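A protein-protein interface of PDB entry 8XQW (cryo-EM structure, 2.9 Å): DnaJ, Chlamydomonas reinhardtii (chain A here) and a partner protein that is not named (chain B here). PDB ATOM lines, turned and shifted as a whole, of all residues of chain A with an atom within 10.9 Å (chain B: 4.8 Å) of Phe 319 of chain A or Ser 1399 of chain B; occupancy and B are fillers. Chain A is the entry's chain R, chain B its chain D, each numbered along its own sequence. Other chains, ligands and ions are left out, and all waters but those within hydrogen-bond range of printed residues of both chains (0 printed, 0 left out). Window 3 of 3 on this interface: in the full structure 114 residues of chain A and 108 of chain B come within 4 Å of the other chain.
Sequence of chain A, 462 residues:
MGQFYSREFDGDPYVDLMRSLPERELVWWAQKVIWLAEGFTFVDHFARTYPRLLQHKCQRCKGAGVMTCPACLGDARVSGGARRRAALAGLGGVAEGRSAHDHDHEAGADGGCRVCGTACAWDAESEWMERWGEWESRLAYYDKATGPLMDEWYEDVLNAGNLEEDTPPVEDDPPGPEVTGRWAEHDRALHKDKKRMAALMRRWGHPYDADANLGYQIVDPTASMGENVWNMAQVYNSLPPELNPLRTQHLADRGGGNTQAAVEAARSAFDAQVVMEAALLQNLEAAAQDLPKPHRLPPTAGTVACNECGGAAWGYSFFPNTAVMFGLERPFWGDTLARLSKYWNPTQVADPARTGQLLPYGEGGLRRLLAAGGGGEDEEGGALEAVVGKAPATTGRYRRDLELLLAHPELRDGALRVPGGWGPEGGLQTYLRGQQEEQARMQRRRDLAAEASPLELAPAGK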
ATOM      1  N   TYR A  50      -6.432  20.928  22.860  1.00  0.00           N
ATOM      2  CA  TYR A  50      -7.339  20.245  23.773  1.00  0.00           C
ATOM      3  C   TYR A  50      -7.748  21.092  24.964  1.00  0.00           C
ATOM      4  O   TYR A  50      -8.945  21.092  25.296  1.00  0.00           O
ATOM      5  CB  TYR A  50      -6.722  18.930  24.240  1.00  0.00           C
ATOM      6  CG  TYR A  50      -7.666  18.089  25.050  1.00  0.00           C
ATOM      7  CD1 TYR A  50      -8.734  17.446  24.456  1.00  0.00           C
ATOM      8  CD2 TYR A  50      -7.489  17.936  26.409  1.00  0.00           C
ATOM      9  CE1 TYR A  50      -9.593  16.675  25.192  1.00  0.00           C
ATOM     10  CE2 TYR A  50      -8.345  17.166  27.150  1.00  0.00           C
ATOM     11  CZ  TYR A  50      -9.392  16.540  26.537  1.00  0.00           C
ATOM     12  OH  TYR A  50     -10.247  15.779  27.279  1.00  0.00           O
ATOM     13  N   PRO A  51      -6.859  21.818  25.645  1.00  0.00           N
ATOM     14  CA  PRO A  51      -7.299  22.621  26.788  1.00  0.00           C
ATOM     15  C   PRO A  51      -8.360  23.647  26.474  1.00  0.00           C
ATOM     16  O   PRO A  51      -8.843  24.290  27.403  1.00  0.00           O
ATOM     17  CB  PRO A  51      -6.010  23.300  27.240  1.00  0.00           C
ATOM     18  CG  PRO A  51      -4.994  22.352  26.900  1.00  0.00           C
ATOM     19  CD  PRO A  51      -5.393  21.763  25.598  1.00  0.00           C
ATOM     20  N   ARG A  52      -8.737  23.842  25.220  1.00  0.00           N
ATOM     21  CA  ARG A  52      -9.756  24.835  24.936  1.00  0.00           C
ATOM     22  C   ARG A  52     -11.149  24.366  25.303  1.00  0.00           C
ATOM     23  O   ARG A  52     -12.069  25.182  25.327  1.00  0.00           O
ATOM     24  CB  ARG A  52      -9.725  25.223  23.466  1.00  0.00           C
ATOM     25  CG  ARG A  52      -8.482  25.953  23.081  1.00  0.00           C
ATOM     26  CD  ARG A  52      -8.619  26.571  21.718  1.00  0.00           C
ATOM     27  NE  ARG A  52      -7.324  27.017  21.224  1.00  0.00           N
ATOM     28  CZ  ARG A  52      -7.130  27.577  20.039  1.00  0.00           C
ATOM     29  NH1 ARG A  52      -8.152  27.770  19.220  1.00  0.00           N
ATOM     30  NH2 ARG A  52      -5.912  27.948  19.680  1.00  0.00           N
ATOM     31  N   LEU A  53     -11.335  23.079  25.574  1.00  0.00           N
ATOM     32  CA  LEU A  53     -12.650  22.620  25.988  1.00  0.00           C
ATOM     33  C   LEU A  53     -12.868  22.792  27.472  1.00  0.00           C
ATOM     34  O   LEU A  53     -14.012  22.870  27.905  1.00  0.00           O
ATOM     35  CB  LEU A  53     -12.863  21.155  25.644  1.00  0.00           C
ATOM     36  CG  LEU A  53     -12.260  20.623  24.360  1.00  0.00           C
ATOM     37  CD1 LEU A  53     -12.479  19.144  24.303  1.00  0.00           C
ATOM     38  CD2 LEU A  53     -12.896  21.293  23.180  1.00  0.00           C
ATOM     39  N   LEU A  54     -11.809  22.854  28.262  1.00  0.00           N
ATOM     40  CA  LEU A  54     -11.939  22.914  29.702  1.00  0.00           C
ATOM     41  C   LEU A  54     -11.995  24.328  30.244  1.00  0.00           C
ATOM     42  O   LEU A  54     -12.056  24.493  31.458  1.00  0.00           O
ATOM     43  CB  LEU A  54     -10.788  22.161  30.353  1.00  0.00           C
ATOM     44  CG  LEU A  54     -10.422  20.847  29.686  1.00  0.00           C
ATOM     45  CD1 LEU A  54      -9.038  20.462  30.090  1.00  0.00           C
ATOM     46  CD2 LEU A  54     -11.386  19.782  30.094  1.00  0.00           C
ATOM     47  N   GLN A  55     -11.991  25.345  29.395  1.00  0.00           N
ATOM     48  CA  GLN A  55     -12.043  26.727  29.842  1.00  0.00           C
ATOM     49  C   GLN A  55     -13.483  27.156  30.068  1.00  0.00           C
ATOM     50  O   GLN A  55     -14.290  27.128  29.141  1.00  0.00           O
ATOM     51  CB  GLN A  55     -11.406  27.655  28.818  1.00  0.00           C
ATOM     52  CG  GLN A  55      -9.950  27.445  28.592  1.00  0.00           C
ATOM     53  CD  GLN A  55      -9.420  28.358  27.517  1.00  0.00           C
ATOM     54  OE1 GLN A  55     -10.173  29.095  26.896  1.00  0.00           O
ATOM     55  NE2 GLN A  55      -8.120  28.312  27.288  1.00  0.00           N
ATOM     56  N   HIS A  56     -13.798  27.575  31.284  1.00  0.00           N
ATOM     57  CA  HIS A  56     -15.103  28.122  31.598  1.00  0.00           C
ATOM     58  C   HIS A  56     -14.948  29.564  32.025  1.00  0.00           C
ATOM     59  O   HIS A  56     -13.891  29.958  32.501  1.00  0.00           O
ATOM     60  CB  HIS A  56     -15.792  27.369  32.708  1.00  0.00           C
ATOM     61  CG  HIS A  56     -15.897  25.901  32.477  1.00  0.00           C
ATOM     62  ND1 HIS A  56     -17.094  25.275  32.227  1.00  0.00           N
ATOM     63  CD2 HIS A  56     -14.959  24.932  32.486  1.00  0.00           C
ATOM     64  CE1 HIS A  56     -16.885  23.984  32.076  1.00  0.00           C
ATOM     65  NE2 HIS A  56     -15.598  23.749  32.233  1.00  0.00           N
ATOM     66  N   LYS A  57     -16.012  30.340  31.875  1.00  0.00           N
ATOM     67  CA  LYS A  57     -15.998  31.765  32.146  1.00  0.00           C
ATOM     68  C   LYS A  57     -17.016  32.123  33.212  1.00  0.00           C
ATOM     69  O   LYS A  57     -18.019  31.435  33.386  1.00  0.00           O
ATOM     70  CB  LYS A  57     -16.298  32.557  30.894  1.00  0.00           C
ATOM     71  CG  LYS A  57     -15.226  32.444  29.859  1.00  0.00           C
ATOM     72  CD  LYS A  57     -15.527  33.310  28.677  1.00  0.00           C
ATOM     73  CE  LYS A  57     -16.993  33.252  28.346  1.00  0.00           C
ATOM     74  NZ  LYS A  57     -17.304  33.931  27.068  1.00  0.00           N
ATOM     75  N   GLY A 315     -11.465  30.081  34.119  1.00  0.00           N
ATOM     76  CA  GLY A 315     -10.649  29.052  34.736  1.00  0.00           C
ATOM     77  C   GLY A 315     -10.751  27.736  34.004  1.00  0.00           C
ATOM     78  O   GLY A 315     -11.416  27.623  32.978  1.00  0.00           O
ATOM     79  N   TYR A 316     -10.068  26.734  34.550  1.00  0.00           N
ATOM     80  CA  TYR A 316     -10.090  25.368  34.049  1.00  0.00           C
ATOM     81  C   TYR A 316     -10.849  24.486  35.026  1.00  0.00           C
ATOM     82  O   TYR A 316     -10.794  24.706  36.235  1.00  0.00           O
ATOM     83  CB  TYR A 316      -8.681  24.820  33.881  1.00  0.00           C
ATOM     84  CG  TYR A 316      -7.901  25.436  32.767  1.00  0.00           C
ATOM     85  CD1 TYR A 316      -8.083  25.024  31.472  1.00  0.00           C
ATOM     86  CD2 TYR A 316      -6.972  26.423  33.011  1.00  0.00           C
ATOM     87  CE1 TYR A 316      -7.376  25.582  30.455  1.00  0.00           C
ATOM     88  CE2 TYR A 316      -6.258  26.981  31.999  1.00  0.00           C
ATOM     89  CZ  TYR A 316      -6.467  26.559  30.723  1.00  0.00           C
ATOM     90  OH  TYR A 316      -5.758  27.115  29.696  1.00  0.00           O
ATOM     91  N   SER A 317     -11.558  23.477  34.518  1.00  0.00           N
ATOM     92  CA  SER A 317     -12.504  22.804  35.393  1.00  0.00           C
ATOM     93  C   SER A 317     -12.616  21.294  35.306  1.00  0.00           C
ATOM     94  O   SER A 317     -13.399  20.735  36.075  1.00  0.00           O
ATOM     95  CB  SER A 317     -13.899  23.359  35.165  1.00  0.00           C
ATOM     96  OG  SER A 317     -14.804  22.790  36.085  1.00  0.00           O
ATOM     97  N   PHE A 318     -11.944  20.626  34.381  1.00  0.00           N
ATOM     98  CA  PHE A 318     -12.035  19.171  34.265  1.00  0.00           C
ATOM     99  C   PHE A 318     -13.409  18.723  33.762  1.00  0.00           C
ATOM    100  O   PHE A 318     -13.581  17.571  33.365  1.00  0.00           O
ATOM    101  CB  PHE A 318     -11.695  18.501  35.601  1.00  0.00           C
ATOM    102  CG  PHE A 318     -12.216  17.110  35.734  1.00  0.00           C
ATOM    103  CD1 PHE A 318     -11.551  16.054  35.151  1.00  0.00           C
ATOM    104  CD2 PHE A 318     -13.377  16.854  36.430  1.00  0.00           C
ATOM    105  CE1 PHE A 318     -12.031  14.767  35.259  1.00  0.00           C
ATOM    106  CE2 PHE A 318     -13.863  15.567  36.542  1.00  0.00           C
ATOM    107  CZ  PHE A 318     -13.189  14.523  35.954  1.00  0.00           C
ATOM    108  N   PHE A 319     -14.373  19.629  33.709  1.00  0.00           N
ATOM    109  CA  PHE A 319     -15.657  19.393  33.071  1.00  0.00           C
ATOM    110  C   PHE A 319     -15.667  20.044  31.699  1.00  0.00           C
ATOM    111  O   PHE A 319     -15.313  21.213  31.568  1.00  0.00           O
ATOM    112  CB  PHE A 319     -16.798  19.962  33.906  1.00  0.00           C
ATOM    113  CG  PHE A 319     -17.037  19.237  35.187  1.00  0.00           C
ATOM    114  CD1 PHE A 319     -17.156  17.871  35.212  1.00  0.00           C
ATOM    115  CD2 PHE A 319     -17.158  19.925  36.369  1.00  0.00           C
ATOM    116  CE1 PHE A 319     -17.378  17.208  36.391  1.00  0.00           C
ATOM    117  CE2 PHE A 319     -17.384  19.265  37.547  1.00  0.00           C
ATOM    118  CZ  PHE A 319     -17.494  17.908  37.555  1.00  0.00           C
ATOM    119  N   PRO A 320     -16.083  19.342  30.651  1.00  0.00           N
ATOM    120  CA  PRO A 320     -15.690  19.718  29.293  1.00  0.00           C
ATOM    121  C   PRO A 320     -16.329  20.957  28.685  1.00  0.00           C
ATOM    122  O   PRO A 320     -16.002  21.254  27.535  1.00  0.00           O
ATOM    123  CB  PRO A 320     -16.092  18.479  28.496  1.00  0.00           C
ATOM    124  CG  PRO A 320     -16.062  17.403  29.463  1.00  0.00           C
ATOM    125  CD  PRO A 320     -16.645  17.993  30.680  1.00  0.00           C
ATOM    126  N   ASN A 321     -17.214  21.688  29.355  1.00  0.00           N
ATOM    127  CA  ASN A 321     -17.746  22.931  28.792  1.00  0.00           C
ATOM    128  C   ASN A 321     -18.374  22.686  27.417  1.00  0.00           C
ATOM    129  O   ASN A 321     -17.836  23.044  26.377  1.00  0.00           O
ATOM    130  CB  ASN A 321     -16.668  24.011  28.719  1.00  0.00           C
ATOM    131  CG  ASN A 321     -17.155  25.273  28.078  1.00  0.00           C
ATOM    132  OD1 ASN A 321     -16.465  25.865  27.275  1.00  0.00           O
ATOM    133  ND2 ASN A 321     -18.351  25.693  28.426  1.00  0.00           N
ATOM    134  N   THR A 322     -19.513  22.001  27.458  1.00  0.00           N
ATOM    135  CA  THR A 322     -20.233  21.581  26.263  1.00  0.00           C
ATOM    136  C   THR A 322     -20.521  22.710  25.284  1.00  0.00           C
ATOM    137  O   THR A 322     -20.657  22.446  24.088  1.00  0.00           O
ATOM    138  CB  THR A 322     -21.543  20.945  26.681  1.00  0.00           C
ATOM    139  OG1 THR A 322     -22.334  21.929  27.344  1.00  0.00           O
ATOM    140  CG2 THR A 322     -21.284  19.823  27.641  1.00  0.00           C
ATOM    141  N   ALA A 323     -20.631  23.952  25.744  1.00  0.00           N
ATOM    142  CA  ALA A 323     -20.964  25.037  24.829  1.00  0.00           C
ATOM    143  C   ALA A 323     -19.886  25.228  23.779  1.00  0.00           C
ATOM    144  O   ALA A 323     -20.181  25.589  22.639  1.00  0.00           O
ATOM    145  CB  ALA A 323     -21.187  26.328  25.601  1.00  0.00           C
ATOM    146  N   VAL A 324     -18.629  24.994  24.142  1.00  0.00           N
ATOM    147  CA  VAL A 324     -17.549  25.018  23.168  1.00  0.00           C
ATOM    148  C   VAL A 324     -17.537  23.744  22.344  1.00  0.00           C
ATOM    149  O   VAL A 324     -17.311  23.780  21.131  1.00  0.00           O
ATOM    150  CB  VAL A 324     -16.213  25.225  23.892  1.00  0.00           C
ATOM    151  CG1 VAL A 324     -15.074  24.783  23.031  1.00  0.00           C
ATOM    152  CG2 VAL A 324     -16.053  26.664  24.255  1.00  0.00           C
ATOM    153  N   MET A 325     -17.798  22.604  22.978  1.00  0.00           N
ATOM    154  CA  MET A 325     -17.694  21.322  22.300  1.00  0.00           C
ATOM    155  C   MET A 325     -18.730  21.187  21.196  1.00  0.00           C
ATOM    156  O   MET A 325     -18.510  20.472  20.217  1.00  0.00           O
ATOM    157  CB  MET A 325     -17.844  20.197  23.316  1.00  0.00           C
ATOM    158  CG  MET A 325     -17.396  18.855  22.822  1.00  0.00           C
ATOM    159  SD  MET A 325     -18.115  17.517  23.777  1.00  0.00           S
ATOM    160  CE  MET A 325     -18.193  18.297  25.378  1.00  0.00           C
ATOM    161  N   PHE A 326     -19.873  21.848  21.336  1.00  0.00           N
ATOM    162  CA  PHE A 326     -20.894  21.810  20.299  1.00  0.00           C
ATOM    163  C   PHE A 326     -21.004  23.118  19.541  1.00  0.00           C
ATOM    164  O   PHE A 326     -21.792  23.210  18.603  1.00  0.00           O
ATOM    165  CB  PHE A 326     -22.246  21.431  20.895  1.00  0.00           C
ATOM    166  CG  PHE A 326     -22.251  20.090  21.546  1.00  0.00           C
ATOM    167  CD1 PHE A 326     -21.872  18.970  20.847  1.00  0.00           C
ATOM    168  CD2 PHE A 326     -22.615  19.948  22.859  1.00  0.00           C
ATOM    169  CE1 PHE A 326     -21.856  17.748  21.448  1.00  0.00           C
ATOM    170  CE2 PHE A 326     -22.598  18.723  23.454  1.00  0.00           C
ATOM    171  CZ  PHE A 326     -22.221  17.627  22.748  1.00  0.00           C
ATOM    172  N   ASN B1364     -16.951  25.063  39.291  1.00  0.00           N
ATOM    173  CA  ASN B1364     -17.597  23.811  39.662  1.00  0.00           C
ATOM    174  C   ASN B1364     -18.868  24.073  40.443  1.00  0.00           C
ATOM    175  O   ASN B1364     -19.878  23.380  40.259  1.00  0.00           O
ATOM    176  CB  ASN B1364     -16.645  22.946  40.473  1.00  0.00           C
ATOM    177  CG  ASN B1364     -15.497  22.423  39.654  1.00  0.00           C
ATOM    178  OD1 ASN B1364     -14.656  21.684  40.151  1.00  0.00           O
ATOM    179  ND2 ASN B1364     -15.453  22.802  38.394  1.00  0.00           N
ATOM    180  N   ILE B1367     -21.559  24.880  37.812  1.00  0.00           N
ATOM    181  CA  ILE B1367     -21.951  23.709  37.026  1.00  0.00           C
ATOM    182  C   ILE B1367     -22.904  22.832  37.821  1.00  0.00           C
ATOM    183  O   ILE B1367     -24.020  22.509  37.381  1.00  0.00           O
ATOM    184  CB  ILE B1367     -20.706  22.920  36.597  1.00  0.00           C
ATOM    185  CG1 ILE B1367     -19.863  23.740  35.630  1.00  0.00           C
ATOM    186  CG2 ILE B1367     -21.104  21.617  35.973  1.00  0.00           C
ATOM    187  CD1 ILE B1367     -18.568  23.088  35.278  1.00  0.00           C
ATOM    188  N   LEU B1395     -22.937  12.990  34.830  1.00  0.00           N
ATOM    189  CA  LEU B1395     -21.976  14.042  34.525  1.00  0.00           C
ATOM    190  C   LEU B1395     -20.546  13.577  34.752  1.00  0.00           C
ATOM    191  O   LEU B1395     -19.699  13.659  33.851  1.00  0.00           O
ATOM    192  CB  LEU B1395     -22.292  15.260  35.380  1.00  0.00           C
ATOM    193  CG  LEU B1395     -21.431  16.500  35.262  1.00  0.00           C
ATOM    194  CD1 LEU B1395     -21.325  16.917  33.827  1.00  0.00           C
ATOM    195  CD2 LEU B1395     -22.056  17.591  36.078  1.00  0.00           C
ATOM    196  N   MET B1396     -20.258  13.086  35.956  1.00  0.00           N
ATOM    197  CA  MET B1396     -18.896  12.664  36.269  1.00  0.00           C
ATOM    198  C   MET B1396     -18.433  11.542  35.353  1.00  0.00           C
ATOM    199  O   MET B1396     -17.300  11.567  34.843  1.00  0.00           O
ATOM    200  CB  MET B1396     -18.812  12.235  37.725  1.00  0.00           C
ATOM    201  CG  MET B1396     -19.268  13.313  38.675  1.00  0.00           C
ATOM    202  SD  MET B1396     -18.659  13.111  40.352  1.00  0.00           S
ATOM    203  CE  MET B1396     -19.163  11.430  40.690  1.00  0.00           C
ATOM    204  N   SER B1397     -19.291  10.549  35.127  1.00  0.00           N
ATOM    205  CA  SER B1397     -18.915   9.428  34.280  1.00  0.00           C
ATOM    206  C   SER B1397     -18.577   9.881  32.869  1.00  0.00           C
ATOM    207  O   SER B1397     -17.547   9.479  32.311  1.00  0.00           O
ATOM    208  CB  SER B1397     -20.043   8.410  34.258  1.00  0.00           C
ATOM    209  OG  SER B1397     -20.106   7.777  33.002  1.00  0.00           O
ATOM    210  N   SER B1398     -19.424  10.715  32.268  1.00  0.00           N
ATOM    211  CA  SER B1398     -19.169  11.116  30.892  1.00  0.00           C
ATOM    212  C   SER B1398     -17.921  11.981  30.784  1.00  0.00           C
ATOM    213  O   SER B1398     -17.194  11.901  29.792  1.00  0.00           O
ATOM    214  CB  SER B1398     -20.382  11.831  30.320  1.00  0.00           C
ATOM    215  OG  SER B1398     -20.928  12.712  31.271  1.00  0.00           O
ATOM    216  N   SER B1399     -17.623  12.783  31.806  1.00  0.00           N
ATOM    217  CA  SER B1399     -16.397  13.577  31.750  1.00  0.00           C
ATOM    218  C   SER B1399     -15.154  12.694  31.766  1.00  0.00           C
ATOM    219  O   SER B1399     -14.241  12.859  30.934  1.00  0.00           O
ATOM    220  CB  SER B1399     -16.370  14.568  32.902  1.00  0.00           C
ATOM    221  OG  SER B1399     -17.623  15.202  33.029  1.00  0.00           O
ATOM    222  N   ILE B1400     -15.085  11.751  32.707  1.00  0.00           N
ATOM    223  CA  ILE B1400     -13.908  10.885  32.759  1.00  0.00           C
ATOM    224  C   ILE B1400     -13.771  10.093  31.470  1.00  0.00           C
ATOM    225  O   ILE B1400     -12.660   9.882  30.963  1.00  0.00           O
ATOM    226  CB  ILE B1400     -13.968   9.950  33.974  1.00  0.00           C
ATOM    227  CG1 ILE B1400     -14.272  10.740  35.235  1.00  0.00           C
ATOM    228  CG2 ILE B1400     -12.657   9.227  34.126  1.00  0.00           C
ATOM    229  CD1 ILE B1400     -14.752   9.880  36.369  1.00  0.00           C
ATOM    230  N   LEU B1401     -14.892   9.634  30.919  1.00  0.00           N
ATOM    231  CA  LEU B1401     -14.810   8.874  29.683  1.00  0.00           C
ATOM    232  C   LEU B1401     -14.330   9.733  28.528  1.00  0.00           C
ATOM    233  O   LEU B1401     -13.618   9.239  27.652  1.00  0.00           O
ATOM    234  CB  LEU B1401     -16.159   8.259  29.353  1.00  0.00           C
ATOM    235  CG  LEU B1401     -16.205   6.743  29.362  1.00  0.00           C
ATOM    236  CD1 LEU B1401     -17.527   6.301  28.816  1.00  0.00           C
ATOM    237  CD2 LEU B1401     -15.087   6.178  28.538  1.00  0.00           C
ATOM    238  N   LEU B1402     -14.703  11.009  28.498  1.00  0.00           N
ATOM    239  CA  LEU B1402     -14.202  11.877  27.442  1.00  0.00           C
ATOM    240  C   LEU B1402     -12.690  11.973  27.492  1.00  0.00           C
ATOM    241  O   LEU B1402     -12.011  11.838  26.469  1.00  0.00           O
ATOM    242  CB  LEU B1402     -14.818  13.263  27.553  1.00  0.00           C
ATOM    243  CG  LEU B1402     -14.634  14.035  26.256  1.00  0.00           C
ATOM    244  CD1 LEU B1402     -15.763  13.721  25.326  1.00  0.00           C
ATOM    245  CD2 LEU B1402     -14.549  15.509  26.505  1.00  0.00           C
ATOM    246  N   HIS B1403     -12.140  12.200  28.684  1.00  0.00           N
ATOM    247  CA  HIS B1403     -10.686  12.324  28.778  1.00  0.00           C
ATOM    248  C   HIS B1403      -9.990  11.032  28.367  1.00  0.00           C
ATOM    249  O   HIS B1403      -8.988  11.058  27.637  1.00  0.00           O
ATOM    250  CB  HIS B1403     -10.270  12.725  30.186  1.00  0.00           C
ATOM    251  CG  HIS B1403     -10.888  14.003  30.647  1.00  0.00           C
ATOM    252  ND1 HIS B1403     -11.156  15.046  29.792  1.00  0.00           N
ATOM    253  CD2 HIS B1403     -11.313  14.396  31.866  1.00  0.00           C
ATOM    254  CE1 HIS B1403     -11.713  16.033  30.468  1.00  0.00           C
ATOM    255  NE2 HIS B1403     -11.820  15.664  31.728  1.00  0.00           N
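A ring nitrogen (ND1) of His 1403 of chain B sits at hydrogen-bond distance from the side-chain hydroxyl (OH) of Tyr 50 of chain A (2.8 Å).
The backbone carbonyl oxygen (O) of Phe 318 of chain A lies within hydrogen-bond range of a ring nitrogen (NE2) of His 1403 of chain B (3.1 Å).
ND2 of Asn 1364 of chain B sits close to OG of Ser 317 of chain A (2.4 Å).
The backbone carbonyl oxygen (O) of Leu 53 of chain A lies close to the backbone carbonyl oxygen (O) of Pro 320 of chain A, 2.6 Å away.
The backbone NH of Ser 317 of chain A is in hydrogen-bond range of the backbone carbonyl oxygen of Leu 54 of chain A (3.3 Å).
O of His 56 of chain A is in hydrogen-bond range of N of Gly 315 of chain A (2.9 Å).
The backbone carbonyl oxygen (O) of Phe 319 of chain A lies within hydrogen-bond range of a ring nitrogen (NE2) of His 56 of chain A, 2.6 Å away.
The backbone carbonyl oxygen (O) of Leu 1395 of chain B sits at hydrogen-bond distance from the side-chain hydroxyl (OG) of Ser 1399 of chain B (2.7 Å).
Among the printed residues, merely in contact across the chains: Phe 319 of chain A with Ser 1399 of chain B (3.5 Å), Phe 319 of chain A with Ile 1367 of chain B (3.6 Å), His 56 of chain A with Ile 1367 of chain B (3.7 Å), Pro 320 of chain A with Ser 1399 of chain B (3.8 Å), Leu 54 of chain A with His 1403 of chain B (3.8 Å), Pro 320 of chain A with Leu 1402 of chain B (3.8 Å), Ser 317 of chain A with Ile 1367 of chain B (3.9 Å) and Phe 319 of chain A with Asn 1364 of chain B (3.9 Å).
Of chain B, only Asn 1364 (3.9 Å), Ile 1367 (3.6 Å) and Ser 1399 (3.5 Å) come within 4 Å of Phe 319 of chain A.
Ser 1399 of chain B touches just these residues of chain A: Phe 319 and Pro 320.
Leu 1395 of chain B touches none of the printed residues of chain A.
No residue of chain A comes within 4 Å of Ser 1397 of chain B.
No residue of chain A comes within 4 Å of Ser 1398 of chain B.
Of chain A, only Pro 320 (3.8 Å) comes within 4 Å of Leu 1402 of chain B.
Printed residues of chain B within 4 Å of Ser 317 of chain A: Asn 1364 and Ile 1367.
Of the printed residues of chain B, Pro 320 of chain A touches Ser 1399 and Leu 1402.
Of the printed residues of chain B, Tyr 50 of chain A touches His 1403.
Phe 326 of chain A touches none of the printed residues of chain B.
Asn 321 of chain A touches none of the printed residues of chain B.
The nearest residue of chain B that does not touch Phe 319 of chain A is Leu 1395 of chain B (4.3 Å).
The nearest residue of chain A that does not touch Ser 1399 of chain B is Phe 318 of chain A (4.1 Å).
The nearest printed residue of chain B that does not touch Phe 318 of chain A is Ile 1400 of chain B (4.0001 Å).
Hydrophobic or aromatic side chains of chain B within 4 Å of the printed part of chain A: Ile 1367, Leu 1402 and His 1403.
Along chain B the printed residues that touch a printed residue of chain A span positions 1364 to 1403.
Printed residues of chain A that touch a printed residue of chain B: Tyr 50, Leu 54, His 56, Ser 317, Phe 318, Phe 319 and Pro 320.
Hydrophobic or aromatic side chains of chain A that line the printed part of chain B: Tyr 50, Leu 54, His 56, Phe 318, Phe 319 and Pro 320.
Among the printed residues, no Asp or Glu carboxylate lies within 4 Å of a Lys or Arg side-chain nitrogen of the other chain.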
